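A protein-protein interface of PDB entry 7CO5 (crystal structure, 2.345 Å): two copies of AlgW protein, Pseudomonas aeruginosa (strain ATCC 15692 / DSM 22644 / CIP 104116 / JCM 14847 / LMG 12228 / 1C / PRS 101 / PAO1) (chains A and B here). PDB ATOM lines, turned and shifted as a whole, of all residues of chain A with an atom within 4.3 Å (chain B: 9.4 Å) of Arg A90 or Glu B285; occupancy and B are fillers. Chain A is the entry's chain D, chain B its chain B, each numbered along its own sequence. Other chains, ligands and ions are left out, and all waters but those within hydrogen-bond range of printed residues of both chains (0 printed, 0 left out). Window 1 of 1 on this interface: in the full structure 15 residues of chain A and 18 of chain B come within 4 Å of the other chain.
Pro A81 touches none of the printed residues of chain B. Of the printed residues of chain B, Phe A88 touches Gly B283, Val B284, Glu B285, Gly B309, Val B310 and Tyr B311. Arg A90 touches just these residues of chain B: Glu B285, Ala B308 and Pro B323. Printed residues of chain B within 4 Å of Phe A91: Pro B323 (3.9 Å) and Gly B324 (3.9 Å). Trp B281 touches none of the printed residues of chain A. Glu B285 touches just these residues of chain A: Phe A88 and Arg A90.
No position is printed for both chains. Of the 14 pairs that touch across the chains among the printed residues, none has its exchanged pair printed and touching as well.
N of Ala B308 is in hydrogen-bond range of O of Glu B285 (2.8 Å). The backbone NH of Glu B285 lies within hydrogen-bond range of the backbone carbonyl oxygen of Gly B309, 3.1 Å away. N of Tyr B311 is in hydrogen-bond range of O of Gly B283, 2.7 Å away. The side-chain carboxylate (OD2) of Asp A84 is in salt-bridge range of the guanidinium group (NE) of Arg A89 (3.6 Å). The guanidinium group (NH1) of Arg A90 lies close to the backbone carbonyl oxygen (O) of Phe A83, 3.2 Å away. OD2 of Asp A85 is in salt-bridge range of NH1 of Arg A90 (3.5 Å).
NH2 of Arg A90 lies within salt-bridge range of OE1 of Glu B285 (3.1 Å). N of Arg A89 sits at hydrogen-bond distance from O of Val B310, 2.6 Å away.
Printed residues of chain A that touch a printed residue of chain B: Phe A88, Arg A89, Arg A90 and Phe A91. Hydrophobic or aromatic side chains of chain A within 4 Å of the printed part of chain B: Phe A88 and Phe A91. Hydrophobic or aromatic side chains of chain B that line the printed part of chain A: Val B310, Tyr B311 and Pro B323. Among the printed residues, 14 pairs touch across the chains. Among the printed residues, Asp or Glu carboxylates within 4 Å of a Lys or Arg side-chain nitrogen of the other chain: Arg A90 with Glu B285.
Among the printed residues, pairs that only touch across the chains: Phe A88 with Gly B283 (3.8 Å), Phe A88 with Val B284 (3.6 Å), Phe A88 with Glu B285 (3.4 Å), Phe A88 with Gly B309 (3.6 Å), Phe A88 with Val B310 (3.3 Å), Phe A88 with Tyr B311 (3.1 Å), Arg A89 with Gly B309 (3.0 Å), Arg A89 with Pro B323 (3.4 Å), Arg A90 with Ala B308 (3.3 Å), Arg A90 with Pro B323 (3.9 Å), Phe A91 with Pro B323 (3.9 Å) and Phe A91 with Gly B324 (3.9 Å).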
ATOM      1  N   SER A  79      14.933 -13.140 -19.331  1.00  0.00           N
ATOM      2  CA  SER A  79      13.641 -13.463 -20.002  1.00  0.00           C
ATOM      3  C   SER A  79      13.735 -14.517 -21.108  1.00  0.00           C
ATOM      4  O   SER A  79      14.751 -14.592 -21.785  1.00  0.00           O
ATOM      5  CB  SER A  79      12.930 -12.220 -20.494  1.00  0.00           C
ATOM      6  OG  SER A  79      11.645 -12.530 -20.996  1.00  0.00           O
ATOM      7  N   PRO A  81      10.628 -16.476 -23.945  1.00  0.00           N
ATOM      8  CA  PRO A  81       9.294 -16.173 -24.475  1.00  0.00           C
ATOM      9  C   PRO A  81       7.959 -16.670 -23.902  1.00  0.00           C
ATOM     10  O   PRO A  81       7.050 -15.897 -23.949  1.00  0.00           O
ATOM     11  CB  PRO A  81       9.425 -16.715 -25.902  1.00  0.00           C
ATOM     12  CG  PRO A  81      10.856 -16.441 -26.225  1.00  0.00           C
ATOM     13  CD  PRO A  81      11.527 -16.964 -24.980  1.00  0.00           C
ATOM     14  N   LEU A  82       7.827 -17.908 -23.437  1.00  0.00           N
ATOM     15  CA  LEU A  82       6.475 -18.313 -22.968  1.00  0.00           C
ATOM     16  C   LEU A  82       6.383 -18.274 -21.442  1.00  0.00           C
ATOM     17  O   LEU A  82       5.349 -18.691 -20.913  1.00  0.00           O
ATOM     18  CB  LEU A  82       6.153 -19.698 -23.531  1.00  0.00           C
ATOM     19  CG  LEU A  82       6.566 -19.881 -24.988  1.00  0.00           C
ATOM     20  CD1 LEU A  82       6.629 -21.347 -25.373  1.00  0.00           C
ATOM     21  CD2 LEU A  82       5.657 -19.112 -25.923  1.00  0.00           C
ATOM     22  N   PHE A  83       7.411 -17.735 -20.788  1.00  0.00           N
ATOM     23  CA  PHE A  83       7.497 -17.691 -19.308  1.00  0.00           C
ATOM     24  C   PHE A  83       7.076 -16.326 -18.768  1.00  0.00           C
ATOM     25  O   PHE A  83       7.604 -15.349 -19.238  1.00  0.00           O
ATOM     26  CB  PHE A  83       8.912 -18.074 -18.887  1.00  0.00           C
ATOM     27  CG  PHE A  83       9.049 -19.539 -18.589  1.00  0.00           C
ATOM     28  CD1 PHE A  83       8.451 -20.477 -19.406  1.00  0.00           C
ATOM     29  CD2 PHE A  83       9.755 -19.976 -17.490  1.00  0.00           C
ATOM     30  CE1 PHE A  83       8.550 -21.825 -19.126  1.00  0.00           C
ATOM     31  CE2 PHE A  83       9.853 -21.324 -17.218  1.00  0.00           C
ATOM     32  CZ  PHE A  83       9.265 -22.247 -18.041  1.00  0.00           C
ATOM     33  N   ASP A  84       6.256 -16.308 -17.716  1.00  0.00           N
ATOM     34  CA  ASP A  84       5.721 -15.051 -17.132  1.00  0.00           C
ATOM     35  C   ASP A  84       6.872 -14.132 -16.756  1.00  0.00           C
ATOM     36  O   ASP A  84       7.852 -14.592 -16.173  1.00  0.00           O
ATOM     37  CB  ASP A  84       4.966 -15.285 -15.828  1.00  0.00           C
ATOM     38  CG  ASP A  84       3.594 -15.901 -16.000  1.00  0.00           C
ATOM     39  OD1 ASP A  84       3.530 -17.066 -16.396  1.00  0.00           O
ATOM     40  OD2 ASP A  84       2.612 -15.214 -15.725  1.00  0.00           O
ATOM     41  N   ASP A  85       6.682 -12.853 -17.051  1.00  0.00           N
ATOM     42  CA  ASP A  85       7.670 -11.771 -16.860  1.00  0.00           C
ATOM     43  C   ASP A  85       7.288 -10.926 -15.645  1.00  0.00           C
ATOM     44  O   ASP A  85       6.264 -11.190 -15.044  1.00  0.00           O
ATOM     45  CB  ASP A  85       7.651 -10.909 -18.116  1.00  0.00           C
ATOM     46  CG  ASP A  85       8.962 -10.244 -18.421  1.00  0.00           C
ATOM     47  OD1 ASP A  85       9.845 -10.354 -17.582  1.00  0.00           O
ATOM     48  OD2 ASP A  85       9.070  -9.636 -19.497  1.00  0.00           O
ATOM     49  N   PHE A  88       4.871  -8.666 -17.596  1.00  0.00           N
ATOM     50  CA  PHE A  88       3.922  -9.322 -18.540  1.00  0.00           C
ATOM     51  C   PHE A  88       3.547 -10.738 -18.106  1.00  0.00           C
ATOM     52  O   PHE A  88       4.304 -11.389 -17.407  1.00  0.00           O
ATOM     53  CB  PHE A  88       4.498  -9.381 -19.954  1.00  0.00           C
ATOM     54  CG  PHE A  88       4.158  -8.205 -20.826  1.00  0.00           C
ATOM     55  CD1 PHE A  88       4.829  -7.010 -20.696  1.00  0.00           C
ATOM     56  CD2 PHE A  88       3.176  -8.294 -21.786  1.00  0.00           C
ATOM     57  CE1 PHE A  88       4.522  -5.926 -21.498  1.00  0.00           C
ATOM     58  CE2 PHE A  88       2.862  -7.208 -22.586  1.00  0.00           C
ATOM     59  CZ  PHE A  88       3.535  -6.023 -22.442  1.00  0.00           C
ATOM     60  N   ARG A  89       2.389 -11.196 -18.574  1.00  0.00           N
ATOM     61  CA  ARG A  89       1.845 -12.528 -18.237  1.00  0.00           C
ATOM     62  C   ARG A  89       1.933 -13.438 -19.457  1.00  0.00           C
ATOM     63  O   ARG A  89       1.745 -12.954 -20.563  1.00  0.00           O
ATOM     64  CB  ARG A  89       0.381 -12.389 -17.850  1.00  0.00           C
ATOM     65  CG  ARG A  89      -0.007 -13.238 -16.657  1.00  0.00           C
ATOM     66  CD  ARG A  89       0.581 -12.625 -15.407  1.00  0.00           C
ATOM     67  NE  ARG A  89       0.146 -13.171 -14.137  1.00  0.00           N
ATOM     68  CZ  ARG A  89      -1.023 -13.742 -13.903  1.00  0.00           C
ATOM     69  NH1 ARG A  89      -1.941 -13.840 -14.850  1.00  0.00           N
ATOM     70  NH2 ARG A  89      -1.280 -14.195 -12.692  1.00  0.00           N
ATOM     71  N   ARG A  90       2.165 -14.727 -19.213  1.00  0.00           N
ATOM     72  CA  ARG A  90       2.308 -15.754 -20.271  1.00  0.00           C
ATOM     73  C   ARG A  90       1.794 -17.090 -19.741  1.00  0.00           C
ATOM     74  O   ARG A  90       1.446 -17.175 -18.566  1.00  0.00           O
ATOM     75  CB  ARG A  90       3.760 -15.837 -20.734  1.00  0.00           C
ATOM     76  CG  ARG A  90       4.154 -14.714 -21.676  1.00  0.00           C
ATOM     77  CD  ARG A  90       5.607 -14.371 -21.525  1.00  0.00           C
ATOM     78  NE  ARG A  90       5.908 -13.163 -22.260  1.00  0.00           N
ATOM     79  CZ  ARG A  90       6.855 -12.316 -21.920  1.00  0.00           C
ATOM     80  NH1 ARG A  90       7.578 -12.539 -20.841  1.00  0.00           N
ATOM     81  NH2 ARG A  90       7.064 -11.238 -22.642  1.00  0.00           N
ATOM     82  N   PHE A  91       1.749 -18.093 -20.603  1.00  0.00           N
ATOM     83  CA  PHE A  91       1.182 -19.416 -20.255  1.00  0.00           C
ATOM     84  C   PHE A  91       1.940 -20.080 -19.102  1.00  0.00           C
ATOM     85  O   PHE A  91       1.275 -20.666 -18.253  1.00  0.00           O
ATOM     86  CB  PHE A  91       1.167 -20.306 -21.496  1.00  0.00           C
ATOM     87  CG  PHE A  91       1.201 -19.573 -22.808  1.00  0.00           C
ATOM     88  CD1 PHE A  91       2.298 -18.816 -23.168  1.00  0.00           C
ATOM     89  CD2 PHE A  91       0.149 -19.672 -23.695  1.00  0.00           C
ATOM     90  CE1 PHE A  91       2.328 -18.155 -24.384  1.00  0.00           C
ATOM     91  CE2 PHE A  91       0.187 -19.013 -24.909  1.00  0.00           C
ATOM     92  CZ  PHE A  91       1.274 -18.258 -25.253  1.00  0.00           C
ATOM     93  N   PHE A  92       3.265 -19.976 -19.059  1.00  0.00           N
ATOM     94  CA  PHE A  92       3.978 -20.634 -17.936  1.00  0.00           C
ATOM     95  C   PHE A  92       4.756 -19.639 -17.075  1.00  0.00           C
ATOM     96  O   PHE A  92       5.578 -18.868 -17.600  1.00  0.00           O
ATOM     97  CB  PHE A  92       5.007 -21.647 -18.438  1.00  0.00           C
ATOM     98  CG  PHE A  92       4.588 -22.502 -19.599  1.00  0.00           C
ATOM     99  CD1 PHE A  92       3.627 -23.481 -19.449  1.00  0.00           C
ATOM    100  CD2 PHE A  92       5.186 -22.345 -20.836  1.00  0.00           C
ATOM    101  CE1 PHE A  92       3.247 -24.260 -20.525  1.00  0.00           C
ATOM    102  CE2 PHE A  92       4.823 -23.141 -21.902  1.00  0.00           C
ATOM    103  CZ  PHE A  92       3.853 -24.092 -21.745  1.00  0.00           C
ATOM    104  N   TRP B 281      -2.886   2.782 -24.517  1.00  0.00           N
ATOM    105  CA  TRP B 281      -2.227   1.586 -23.961  1.00  0.00           C
ATOM    106  C   TRP B 281      -3.250   0.461 -23.913  1.00  0.00           C
ATOM    107  O   TRP B 281      -4.398   0.724 -23.840  1.00  0.00           O
ATOM    108  CB  TRP B 281      -1.617   1.908 -22.602  1.00  0.00           C
ATOM    109  CG  TRP B 281      -0.848   0.814 -21.930  1.00  0.00           C
ATOM    110  CD1 TRP B 281      -1.127   0.242 -20.732  1.00  0.00           C
ATOM    111  CD2 TRP B 281       0.357   0.185 -22.382  1.00  0.00           C
ATOM    112  NE1 TRP B 281      -0.202  -0.696 -20.416  1.00  0.00           N
ATOM    113  CE2 TRP B 281       0.731  -0.743 -21.402  1.00  0.00           C
ATOM    114  CE3 TRP B 281       1.157   0.315 -23.512  1.00  0.00           C
ATOM    115  CZ2 TRP B 281       1.857  -1.541 -21.528  1.00  0.00           C
ATOM    116  CZ3 TRP B 281       2.256  -0.494 -23.643  1.00  0.00           C
ATOM    117  CH2 TRP B 281       2.606  -1.400 -22.659  1.00  0.00           C
ATOM    118  N   LEU B 282      -2.820  -0.734 -24.218  1.00  0.00           N
ATOM    119  CA  LEU B 282      -3.661  -1.940 -24.133  1.00  0.00           C
ATOM    120  C   LEU B 282      -2.907  -2.944 -23.265  1.00  0.00           C
ATOM    121  O   LEU B 282      -3.559  -3.686 -22.579  1.00  0.00           O
ATOM    122  CB  LEU B 282      -3.825  -2.450 -25.557  1.00  0.00           C
ATOM    123  CG  LEU B 282      -5.180  -3.024 -25.907  1.00  0.00           C
ATOM    124  CD1 LEU B 282      -6.188  -2.669 -24.858  1.00  0.00           C
ATOM    125  CD2 LEU B 282      -5.627  -2.489 -27.226  1.00  0.00           C
ATOM    126  N   GLY B 283      -1.579  -2.756 -23.189  1.00  0.00           N
ATOM    127  CA  GLY B 283      -0.614  -3.623 -22.480  1.00  0.00           C
ATOM    128  C   GLY B 283      -0.529  -5.032 -23.047  1.00  0.00           C
ATOM    129  O   GLY B 283      -0.743  -5.987 -22.274  1.00  0.00           O
ATOM    130  N   VAL B 284      -0.237  -5.167 -24.351  1.00  0.00           N
ATOM    131  CA  VAL B 284      -0.182  -6.516 -24.972  1.00  0.00           C
ATOM    132  C   VAL B 284       1.145  -6.723 -25.687  1.00  0.00           C
ATOM    133  O   VAL B 284       1.693  -5.779 -26.207  1.00  0.00           O
ATOM    134  CB  VAL B 284      -1.333  -6.790 -25.949  1.00  0.00           C
ATOM    135  CG1 VAL B 284      -2.654  -7.060 -25.269  1.00  0.00           C
ATOM    136  CG2 VAL B 284      -1.447  -5.708 -26.993  1.00  0.00           C
ATOM    137  N   GLU B 285       1.638  -7.952 -25.634  1.00  0.00           N
ATOM    138  CA  GLU B 285       2.841  -8.345 -26.387  1.00  0.00           C
ATOM    139  C   GLU B 285       2.283  -9.213 -27.490  1.00  0.00           C
ATOM    140  O   GLU B 285       1.538 -10.081 -27.190  1.00  0.00           O
ATOM    141  CB  GLU B 285       3.881  -9.048 -25.540  1.00  0.00           C
ATOM    142  CG  GLU B 285       4.985  -9.595 -26.407  1.00  0.00           C
ATOM    143  CD  GLU B 285       6.238 -10.107 -25.743  1.00  0.00           C
ATOM    144  OE1 GLU B 285       6.883  -9.333 -25.072  1.00  0.00           O
ATOM    145  OE2 GLU B 285       6.570 -11.259 -25.957  1.00  0.00           O
ATOM    146  N   VAL B 286       2.619  -8.911 -28.729  1.00  0.00           N
ATOM    147  CA  VAL B 286       1.948  -9.590 -29.862  1.00  0.00           C
ATOM    148  C   VAL B 286       2.960 -10.163 -30.848  1.00  0.00           C
ATOM    149  O   VAL B 286       3.987  -9.573 -31.040  1.00  0.00           O
ATOM    150  CB  VAL B 286       1.035  -8.552 -30.536  1.00  0.00           C
ATOM    151  CG1 VAL B 286       0.519  -8.965 -31.888  1.00  0.00           C
ATOM    152  CG2 VAL B 286      -0.094  -8.115 -29.642  1.00  0.00           C
ATOM    153  N   LYS B 287       2.660 -11.327 -31.386  1.00  0.00           N
ATOM    154  CA  LYS B 287       3.463 -11.873 -32.492  1.00  0.00           C
ATOM    155  C   LYS B 287       2.507 -12.247 -33.611  1.00  0.00           C
ATOM    156  O   LYS B 287       1.376 -12.574 -33.318  1.00  0.00           O
ATOM    157  CB  LYS B 287       4.414 -12.999 -32.095  1.00  0.00           C
ATOM    158  CG  LYS B 287       3.883 -14.062 -31.168  1.00  0.00           C
ATOM    159  CD  LYS B 287       5.048 -14.788 -30.559  1.00  0.00           C
ATOM    160  CE  LYS B 287       6.216 -13.870 -30.257  1.00  0.00           C
ATOM    161  NZ  LYS B 287       7.491 -14.596 -30.126  1.00  0.00           N
ATOM    162  N   ALA B 288       2.963 -12.107 -34.844  1.00  0.00           N
ATOM    163  CA  ALA B 288       2.144 -12.449 -36.012  1.00  0.00           C
ATOM    164  C   ALA B 288       1.880 -13.944 -35.970  1.00  0.00           C
ATOM    165  O   ALA B 288       2.800 -14.680 -35.680  1.00  0.00           O
ATOM    166  CB  ALA B 288       2.906 -12.081 -37.238  1.00  0.00           C
ATOM    167  N   ILE B 305      -3.472 -11.754 -35.125  1.00  0.00           N
ATOM    168  CA  ILE B 305      -2.188 -11.485 -34.413  1.00  0.00           C
ATOM    169  C   ILE B 305      -2.279 -12.225 -33.077  1.00  0.00           C
ATOM    170  O   ILE B 305      -3.267 -12.066 -32.411  1.00  0.00           O
ATOM    171  CB  ILE B 305      -1.900  -9.994 -34.224  1.00  0.00           C
ATOM    172  CG1 ILE B 305      -2.979  -9.290 -33.420  1.00  0.00           C
ATOM    173  CG2 ILE B 305      -1.666  -9.301 -35.534  1.00  0.00           C
ATOM    174  CD1 ILE B 305      -2.681  -7.850 -33.212  1.00  0.00           C
ATOM    175  N   VAL B 306      -1.258 -12.953 -32.665  1.00  0.00           N
ATOM    176  CA  VAL B 306      -1.392 -13.750 -31.413  1.00  0.00           C
ATOM    177  C   VAL B 306      -1.067 -12.917 -30.179  1.00  0.00           C
ATOM    178  O   VAL B 306      -0.166 -12.136 -30.230  1.00  0.00           O
ATOM    179  CB  VAL B 306      -0.565 -15.050 -31.443  1.00  0.00           C
ATOM    180  CG1 VAL B 306      -1.023 -16.027 -30.390  1.00  0.00           C
ATOM    181  CG2 VAL B 306      -0.604 -15.740 -32.782  1.00  0.00           C
ATOM    182  N   VAL B 307      -1.780 -13.155 -29.090  1.00  0.00           N
ATOM    183  CA  VAL B 307      -1.477 -12.467 -27.815  1.00  0.00           C
ATOM    184  C   VAL B 307      -0.383 -13.287 -27.148  1.00  0.00           C
ATOM    185  O   VAL B 307      -0.660 -14.366 -26.720  1.00  0.00           O
ATOM    186  CB  VAL B 307      -2.707 -12.334 -26.900  1.00  0.00           C
ATOM    187  CG1 VAL B 307      -2.414 -11.395 -25.753  1.00  0.00           C
ATOM    188  CG2 VAL B 307      -3.934 -11.846 -27.637  1.00  0.00           C
ATOM    189  N   ALA B 308       0.845 -12.817 -27.274  1.00  0.00           N
ATOM    190  CA  ALA B 308       2.058 -13.390 -26.669  1.00  0.00           C
ATOM    191  C   ALA B 308       2.053 -13.178 -25.156  1.00  0.00           C
ATOM    192  O   ALA B 308       2.459 -14.051 -24.454  1.00  0.00           O
ATOM    193  CB  ALA B 308       3.240 -12.750 -27.314  1.00  0.00           C
ATOM    194  N   GLY B 309       1.635 -12.015 -24.696  1.00  0.00           N
ATOM    195  CA  GLY B 309       1.601 -11.717 -23.262  1.00  0.00           C
ATOM    196  C   GLY B 309       0.637 -10.609 -22.954  1.00  0.00           C
ATOM    197  O   GLY B 309       0.186  -9.971 -23.860  1.00  0.00           O
ATOM    198  N   VAL B 310       0.296 -10.446 -21.690  1.00  0.00           N
ATOM    199  CA  VAL B 310      -0.595  -9.347 -21.249  1.00  0.00           C
ATOM    200  C   VAL B 310       0.157  -8.634 -20.140  1.00  0.00           C
ATOM    201  O   VAL B 310       0.708  -9.325 -19.336  1.00  0.00           O
ATOM    202  CB  VAL B 310      -1.948  -9.874 -20.755  1.00  0.00           C
ATOM    203  CG1 VAL B 310      -2.542 -10.869 -21.713  1.00  0.00           C
ATOM    204  CG2 VAL B 310      -1.826 -10.474 -19.375  1.00  0.00           C
ATOM    205  N   TYR B 311       0.159  -7.307 -20.144  1.00  0.00           N
ATOM    206  CA  TYR B 311       0.822  -6.458 -19.131  1.00  0.00           C
ATOM    207  C   TYR B 311       0.090  -6.638 -17.800  1.00  0.00           C
ATOM    208  O   TYR B 311      -1.103  -6.691 -17.817  1.00  0.00           O
ATOM    209  CB  TYR B 311       0.833  -5.029 -19.658  1.00  0.00           C
ATOM    210  CG  TYR B 311       1.803  -4.068 -19.032  1.00  0.00           C
ATOM    211  CD1 TYR B 311       3.112  -4.006 -19.446  1.00  0.00           C
ATOM    212  CD2 TYR B 311       1.389  -3.170 -18.078  1.00  0.00           C
ATOM    213  CE1 TYR B 311       4.000  -3.106 -18.898  1.00  0.00           C
ATOM    214  CE2 TYR B 311       2.260  -2.259 -17.520  1.00  0.00           C
ATOM    215  CZ  TYR B 311       3.572  -2.228 -17.930  1.00  0.00           C
ATOM    216  OH  TYR B 311       4.418  -1.318 -17.385  1.00  0.00           O
ATOM    217  N   ARG B 312       0.826  -6.655 -16.692  1.00  0.00           N
ATOM    218  CA  ARG B 312       0.314  -6.943 -15.335  1.00  0.00           C
ATOM    219  C   ARG B 312      -0.677  -5.869 -14.924  1.00  0.00           C
ATOM    220  O   ARG B 312      -0.327  -4.723 -14.924  1.00  0.00           O
ATOM    221  CB  ARG B 312       1.509  -6.796 -14.399  1.00  0.00           C
ATOM    222  CG  ARG B 312       2.222  -5.458 -14.539  1.00  0.00           C
ATOM    223  CD  ARG B 312       3.589  -5.350 -13.910  1.00  0.00           C
ATOM    224  NE  ARG B 312       4.153  -4.082 -14.318  1.00  0.00           N
ATOM    225  CZ  ARG B 312       4.031  -2.979 -13.608  1.00  0.00           C
ATOM    226  NH1 ARG B 312       3.391  -3.024 -12.455  1.00  0.00           N
ATOM    227  NH2 ARG B 312       4.562  -1.853 -14.034  1.00  0.00           N
ATOM    228  N   ALA B 316      -6.037  -4.403 -21.071  1.00  0.00           N
ATOM    229  CA  ALA B 316      -6.469  -5.685 -21.645  1.00  0.00           C
ATOM    230  C   ALA B 316      -6.536  -6.755 -20.564  1.00  0.00           C
ATOM    231  O   ALA B 316      -7.471  -7.478 -20.566  1.00  0.00           O
ATOM    232  CB  ALA B 316      -5.530  -6.081 -22.743  1.00  0.00           C
ATOM    233  N   LEU B 321      -8.351 -10.500 -21.354  1.00  0.00           N
ATOM    234  CA  LEU B 321      -7.454 -11.000 -22.410  1.00  0.00           C
ATOM    235  C   LEU B 321      -6.502 -12.004 -21.767  1.00  0.00           C
ATOM    236  O   LEU B 321      -5.996 -11.733 -20.692  1.00  0.00           O
ATOM    237  CB  LEU B 321      -6.695  -9.813 -22.995  1.00  0.00           C
ATOM    238  CG  LEU B 321      -6.233 -10.011 -24.425  1.00  0.00           C
ATOM    239  CD1 LEU B 321      -7.298 -10.721 -25.209  1.00  0.00           C
ATOM    240  CD2 LEU B 321      -5.920  -8.697 -25.068  1.00  0.00           C
ATOM    241  N   LEU B 322      -6.281 -13.126 -22.426  1.00  0.00           N
ATOM    242  CA  LEU B 322      -5.393 -14.182 -21.897  1.00  0.00           C
ATOM    243  C   LEU B 322      -4.357 -14.486 -22.960  1.00  0.00           C
ATOM    244  O   LEU B 322      -4.687 -14.395 -24.089  1.00  0.00           O
ATOM    245  CB  LEU B 322      -6.260 -15.403 -21.613  1.00  0.00           C
ATOM    246  CG  LEU B 322      -7.181 -15.219 -20.419  1.00  0.00           C
ATOM    247  CD1 LEU B 322      -8.009 -16.448 -20.160  1.00  0.00           C
ATOM    248  CD2 LEU B 322      -6.376 -14.832 -19.201  1.00  0.00           C
ATOM    249  N   PRO B 323      -3.103 -14.837 -22.657  1.00  0.00           N
ATOM    250  CA  PRO B 323      -2.170 -15.122 -23.712  1.00  0.00           C
ATOM    251  C   PRO B 323      -2.622 -16.333 -24.535  1.00  0.00           C
ATOM    252  O   PRO B 323      -3.171 -17.268 -24.024  1.00  0.00           O
ATOM    253  CB  PRO B 323      -0.828 -15.228 -23.004  1.00  0.00           C
ATOM    254  CG  PRO B 323      -1.072 -14.501 -21.744  1.00  0.00           C
ATOM    255  CD  PRO B 323      -2.483 -14.873 -21.368  1.00  0.00           C
ATOM    256  N   GLY B 324      -2.355 -16.250 -25.828  1.00  0.00           N
ATOM    257  CA  GLY B 324      -2.756 -17.291 -26.782  1.00  0.00           C
ATOM    258  C   GLY B 324      -4.014 -16.892 -27.501  1.00  0.00           C
ATOM    259  O   GLY B 324      -4.385 -17.584 -28.406  1.00  0.00           O
ATOM    260  N   ASP B 325      -4.604 -15.769 -27.118  1.00  0.00           N
ATOM    261  CA  ASP B 325      -5.831 -15.267 -27.779  1.00  0.00           C
ATOM    262  C   ASP B 325      -5.464 -14.759 -29.161  1.00  0.00           C
ATOM    263  O   ASP B 325      -4.373 -14.295 -29.352  1.00  0.00           O
ATOM    264  CB  ASP B 325      -6.534 -14.183 -26.969  1.00  0.00           C
ATOM    265  CG  ASP B 325      -7.350 -14.731 -25.824  1.00  0.00           C
ATOM    266  OD1 ASP B 325      -7.239 -15.908 -25.587  1.00  0.00           O
ATOM    267  OD2 ASP B 325      -8.043 -13.963 -25.163  1.00  0.00           O
ATOM    268  N   ILE B 327      -6.249 -11.994 -31.769  1.00  0.00           N
ATOM    269  CA  ILE B 327      -7.055 -10.765 -31.902  1.00  0.00           C
ATOM    270  C   ILE B 327      -7.558 -10.682 -33.339  1.00  0.00           C
ATOM    271  O   ILE B 327      -6.770 -10.664 -34.231  1.00  0.00           O
ATOM    272  CB  ILE B 327      -6.218  -9.554 -31.504  1.00  0.00           C
ATOM    273  CG1 ILE B 327      -5.853  -9.626 -30.032  1.00  0.00           C
ATOM    274  CG2 ILE B 327      -6.942  -8.271 -31.839  1.00  0.00           C
ATOM    275  CD1 ILE B 327      -5.188  -8.404 -29.538  1.00  0.00           C
ATOM    276  N   GLY B 338       0.529  -6.367 -36.924  1.00  0.00           N
ATOM    277  CA  GLY B 338       0.914  -5.933 -35.572  1.00  0.00           C
ATOM    278  C   GLY B 338       1.297  -4.471 -35.464  1.00  0.00           C
ATOM    279  O   GLY B 338       1.176  -3.950 -34.394  1.00  0.00           O
ATOM    280  N   MET B 342      -0.738  -1.463 -33.528  1.00  0.00           N
ATOM    281  CA  MET B 342       0.065  -0.733 -32.534  1.00  0.00           C
ATOM    282  C   MET B 342      -0.068   0.772 -32.801  1.00  0.00           C
ATOM    283  O   MET B 342      -0.091   1.509 -31.873  1.00  0.00           O
ATOM    284  CB  MET B 342       1.505  -1.238 -32.593  1.00  0.00           C
ATOM    285  CG  MET B 342       2.542  -0.247 -32.225  1.00  0.00           C
ATOM    286  SD  MET B 342       4.061  -1.037 -31.780  1.00  0.00           S
ATOM    287  CE  MET B 342       4.721   0.143 -30.626  1.00  0.00           C
